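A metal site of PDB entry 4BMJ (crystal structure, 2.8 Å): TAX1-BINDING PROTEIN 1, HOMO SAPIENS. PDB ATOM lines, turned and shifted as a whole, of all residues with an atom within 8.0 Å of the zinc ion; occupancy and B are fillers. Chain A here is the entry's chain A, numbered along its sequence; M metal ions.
The zinc ion is bound by NE2 of His 60 (1.9 Å), NE2 of His 56 (1.9 Å), SG of Cys 40 (2.0 Å) and SG of Cys 37 (2.2 Å).
The zinc ion has four donor atoms within binding distance.
O of Glu 42 sits at hydrogen-bond distance from N of Cys 37 (3.0 Å).
SG of Cys 40 sits close to N of Glu 42.
The side-chain sulfur (SG) of Cys 37 lies close to the backbone NH (N) of Met 39, at 3.5 Å.
Four residues have an atom within 4 Å of the zinc ion: Cys 37, Cys 40, His 56 and His 60.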
ATOM      1  N   VAL A  36      23.107 -10.237 -31.429  1.00  0.00           N
ATOM      2  CA  VAL A  36      24.271 -10.866 -32.022  1.00  0.00           C
ATOM      3  C   VAL A  36      25.523 -10.555 -31.233  1.00  0.00           C
ATOM      4  O   VAL A  36      25.830  -9.387 -30.957  1.00  0.00           O
ATOM      5  CB  VAL A  36      24.529 -10.360 -33.460  1.00  0.00           C
ATOM      6  CG1 VAL A  36      25.660 -11.157 -34.106  1.00  0.00           C
ATOM      7  CG2 VAL A  36      23.286 -10.443 -34.262  1.00  0.00           C
ATOM      8  N   CYS A  37      26.263 -11.579 -30.898  1.00  0.00           N
ATOM      9  CA  CYS A  37      27.547 -11.377 -30.318  1.00  0.00           C
ATOM     10  C   CYS A  37      28.474 -10.757 -31.367  1.00  0.00           C
ATOM     11  O   CYS A  37      28.634 -11.317 -32.461  1.00  0.00           O
ATOM     12  CB  CYS A  37      28.106 -12.718 -29.841  1.00  0.00           C
ATOM     13  SG  CYS A  37      29.779 -12.584 -29.260  1.00  0.00           S
ATOM     14  N   PRO A  38      29.058  -9.593 -31.050  1.00  0.00           N
ATOM     15  CA  PRO A  38      29.939  -8.876 -31.975  1.00  0.00           C
ATOM     16  C   PRO A  38      31.277  -9.570 -32.257  1.00  0.00           C
ATOM     17  O   PRO A  38      31.928  -9.253 -33.241  1.00  0.00           O
ATOM     18  CB  PRO A  38      30.201  -7.547 -31.249  1.00  0.00           C
ATOM     19  CG  PRO A  38      29.843  -7.797 -29.826  1.00  0.00           C
ATOM     20  CD  PRO A  38      28.757  -8.809 -29.849  1.00  0.00           C
ATOM     21  N   MET A  39      31.682 -10.508 -31.396  1.00  0.00           N
ATOM     22  CA  MET A  39      32.948 -11.203 -31.614  1.00  0.00           C
ATOM     23  C   MET A  39      32.805 -12.494 -32.427  1.00  0.00           C
ATOM     24  O   MET A  39      33.491 -12.671 -33.418  1.00  0.00           O
ATOM     25  CB  MET A  39      33.619 -11.503 -30.293  1.00  0.00           C
ATOM     26  CG  MET A  39      33.806 -10.276 -29.422  1.00  0.00           C
ATOM     27  SD  MET A  39      35.389  -9.474 -29.713  1.00  0.00           S
ATOM     28  CE  MET A  39      36.531 -10.609 -28.909  1.00  0.00           C
ATOM     29  N   CYS A  40      31.894 -13.381 -32.025  1.00  0.00           N
ATOM     30  CA  CYS A  40      31.755 -14.681 -32.687  1.00  0.00           C
ATOM     31  C   CYS A  40      30.446 -14.829 -33.463  1.00  0.00           C
ATOM     32  O   CYS A  40      30.278 -15.803 -34.183  1.00  0.00           O
ATOM     33  CB  CYS A  40      31.843 -15.808 -31.689  1.00  0.00           C
ATOM     34  SG  CYS A  40      30.412 -15.835 -30.606  1.00  0.00           S
ATOM     35  N   SER A  41      29.529 -13.882 -33.295  1.00  0.00           N
ATOM     36  CA  SER A  41      28.339 -13.839 -34.141  1.00  0.00           C
ATOM     37  C   SER A  41      27.225 -14.776 -33.741  1.00  0.00           C
ATOM     38  O   SER A  41      26.218 -14.840 -34.413  1.00  0.00           O
ATOM     39  CB  SER A  41      28.694 -14.154 -35.581  1.00  0.00           C
ATOM     40  OG  SER A  41      28.860 -12.968 -36.303  1.00  0.00           O
ATOM     41  N   GLU A  42      27.449 -15.539 -32.682  1.00  0.00           N
ATOM     42  CA  GLU A  42      26.391 -16.296 -32.033  1.00  0.00           C
ATOM     43  C   GLU A  42      25.150 -15.405 -31.962  1.00  0.00           C
ATOM     44  O   GLU A  42      25.264 -14.196 -31.840  1.00  0.00           O
ATOM     45  CB  GLU A  42      26.893 -16.661 -30.637  1.00  0.00           C
ATOM     46  CG  GLU A  42      25.906 -17.360 -29.749  1.00  0.00           C
ATOM     47  CD  GLU A  42      25.569 -18.763 -30.231  1.00  0.00           C
ATOM     48  OE1 GLU A  42      26.485 -19.613 -30.393  1.00  0.00           O
ATOM     49  OE2 GLU A  42      24.363 -18.999 -30.452  1.00  0.00           O
ATOM     50  N   GLN A  43      23.966 -15.989 -32.058  1.00  0.00           N
ATOM     51  CA  GLN A  43      22.725 -15.197 -32.037  1.00  0.00           C
ATOM     52  C   GLN A  43      21.827 -15.631 -30.912  1.00  0.00           C
ATOM     53  O   GLN A  43      21.860 -16.810 -30.516  1.00  0.00           O
ATOM     54  CB  GLN A  43      21.990 -15.360 -33.349  1.00  0.00           C
ATOM     55  CG  GLN A  43      22.830 -14.966 -34.538  1.00  0.00           C
ATOM     56  CD  GLN A  43      22.402 -15.659 -35.784  1.00  0.00           C
ATOM     57  OE1 GLN A  43      22.006 -15.019 -36.756  1.00  0.00           O
ATOM     58  NE2 GLN A  43      22.475 -16.973 -35.793  1.00  0.00           N
ATOM     59  N   PHE A  44      21.010 -14.723 -30.386  1.00  0.00           N
ATOM     60  CA  PHE A  44      20.181 -15.083 -29.221  1.00  0.00           C
ATOM     61  C   PHE A  44      18.762 -14.598 -29.378  1.00  0.00           C
ATOM     62  O   PHE A  44      18.479 -13.738 -30.177  1.00  0.00           O
ATOM     63  CB  PHE A  44      20.727 -14.496 -27.906  1.00  0.00           C
ATOM     64  CG  PHE A  44      22.188 -14.746 -27.678  1.00  0.00           C
ATOM     65  CD1 PHE A  44      23.148 -14.030 -28.379  1.00  0.00           C
ATOM     66  CD2 PHE A  44      22.608 -15.686 -26.743  1.00  0.00           C
ATOM     67  CE1 PHE A  44      24.491 -14.278 -28.178  1.00  0.00           C
ATOM     68  CE2 PHE A  44      23.964 -15.935 -26.538  1.00  0.00           C
ATOM     69  CZ  PHE A  44      24.901 -15.247 -27.244  1.00  0.00           C
ATOM     70  N   PHE A  53      23.793 -12.267 -21.621  1.00  0.00           N
ATOM     71  CA  PHE A  53      24.347 -11.945 -22.936  1.00  0.00           C
ATOM     72  C   PHE A  53      25.699 -11.233 -22.844  1.00  0.00           C
ATOM     73  O   PHE A  53      26.671 -11.609 -23.516  1.00  0.00           O
ATOM     74  CB  PHE A  53      23.379 -11.107 -23.783  1.00  0.00           C
ATOM     75  CG  PHE A  53      23.983 -10.605 -25.068  1.00  0.00           C
ATOM     76  CD1 PHE A  53      24.053 -11.418 -26.178  1.00  0.00           C
ATOM     77  CD2 PHE A  53      24.512  -9.320 -25.164  1.00  0.00           C
ATOM     78  CE1 PHE A  53      24.633 -10.950 -27.373  1.00  0.00           C
ATOM     79  CE2 PHE A  53      25.089  -8.875 -26.330  1.00  0.00           C
ATOM     80  CZ  PHE A  53      25.138  -9.674 -27.442  1.00  0.00           C
ATOM     81  N   HIS A  56      28.557 -13.408 -22.052  1.00  0.00           N
ATOM     82  CA  HIS A  56      29.019 -14.239 -23.137  1.00  0.00           C
ATOM     83  C   HIS A  56      30.083 -13.444 -23.867  1.00  0.00           C
ATOM     84  O   HIS A  56      31.200 -13.924 -24.052  1.00  0.00           O
ATOM     85  CB  HIS A  56      27.886 -14.567 -24.096  1.00  0.00           C
ATOM     86  CG  HIS A  56      28.365 -14.976 -25.460  1.00  0.00           C
ATOM     87  ND1 HIS A  56      28.539 -16.294 -25.819  1.00  0.00           N
ATOM     88  CD2 HIS A  56      28.783 -14.226 -26.512  1.00  0.00           C
ATOM     89  CE1 HIS A  56      29.000 -16.346 -27.056  1.00  0.00           C
ATOM     90  NE2 HIS A  56      29.147 -15.099 -27.510  1.00  0.00           N
ATOM     91  N   VAL A  57      29.725 -12.229 -24.260  1.00  0.00           N
ATOM     92  CA  VAL A  57      30.664 -11.376 -24.975  1.00  0.00           C
ATOM     93  C   VAL A  57      31.947 -11.269 -24.177  1.00  0.00           C
ATOM     94  O   VAL A  57      33.023 -11.634 -24.676  1.00  0.00           O
ATOM     95  CB  VAL A  57      30.093  -9.986 -25.255  1.00  0.00           C
ATOM     96  CG1 VAL A  57      31.155  -9.081 -25.830  1.00  0.00           C
ATOM     97  CG2 VAL A  57      28.927 -10.087 -26.216  1.00  0.00           C
ATOM     98  N   GLN A  58      31.828 -10.821 -22.933  1.00  0.00           N
ATOM     99  CA  GLN A  58      32.988 -10.621 -22.070  1.00  0.00           C
ATOM    100  C   GLN A  58      33.938 -11.800 -22.071  1.00  0.00           C
ATOM    101  O   GLN A  58      35.148 -11.629 -22.144  1.00  0.00           O
ATOM    102  CB  GLN A  58      32.556 -10.308 -20.644  1.00  0.00           C
ATOM    103  CG  GLN A  58      33.714  -9.831 -19.776  1.00  0.00           C
ATOM    104  CD  GLN A  58      34.188  -8.456 -20.174  1.00  0.00           C
ATOM    105  OE1 GLN A  58      33.387  -7.532 -20.268  1.00  0.00           O
ATOM    106  NE2 GLN A  58      35.491  -8.315 -20.434  1.00  0.00           N
ATOM    107  N   THR A  59      33.373 -13.003 -22.005  1.00  0.00           N
ATOM    108  CA  THR A  59      34.161 -14.209 -21.943  1.00  0.00           C
ATOM    109  C   THR A  59      35.158 -14.347 -23.084  1.00  0.00           C
ATOM    110  O   THR A  59      36.243 -14.899 -22.921  1.00  0.00           O
ATOM    111  CB  THR A  59      33.265 -15.457 -21.900  1.00  0.00           C
ATOM    112  OG1 THR A  59      32.568 -15.509 -20.649  1.00  0.00           O
ATOM    113  CG2 THR A  59      34.090 -16.727 -22.069  1.00  0.00           C
ATOM    114  N   HIS A  60      34.793 -13.859 -24.267  1.00  0.00           N
ATOM    115  CA  HIS A  60      35.712 -13.918 -25.402  1.00  0.00           C
ATOM    116  C   HIS A  60      37.010 -13.194 -25.013  1.00  0.00           C
ATOM    117  O   HIS A  60      38.113 -13.618 -25.376  1.00  0.00           O
ATOM    118  CB  HIS A  60      35.113 -13.260 -26.647  1.00  0.00           C
ATOM    119  CG  HIS A  60      34.012 -14.043 -27.302  1.00  0.00           C
ATOM    120  ND1 HIS A  60      34.241 -15.210 -28.014  1.00  0.00           N
ATOM    121  CD2 HIS A  60      32.675 -13.815 -27.386  1.00  0.00           C
ATOM    122  CE1 HIS A  60      33.091 -15.659 -28.495  1.00  0.00           C
ATOM    123  NE2 HIS A  60      32.126 -14.837 -28.135  1.00  0.00           N
HETATM  124 ZN    ZN M   1      30.396 -14.721 -28.942  1.00  0.00          ZN
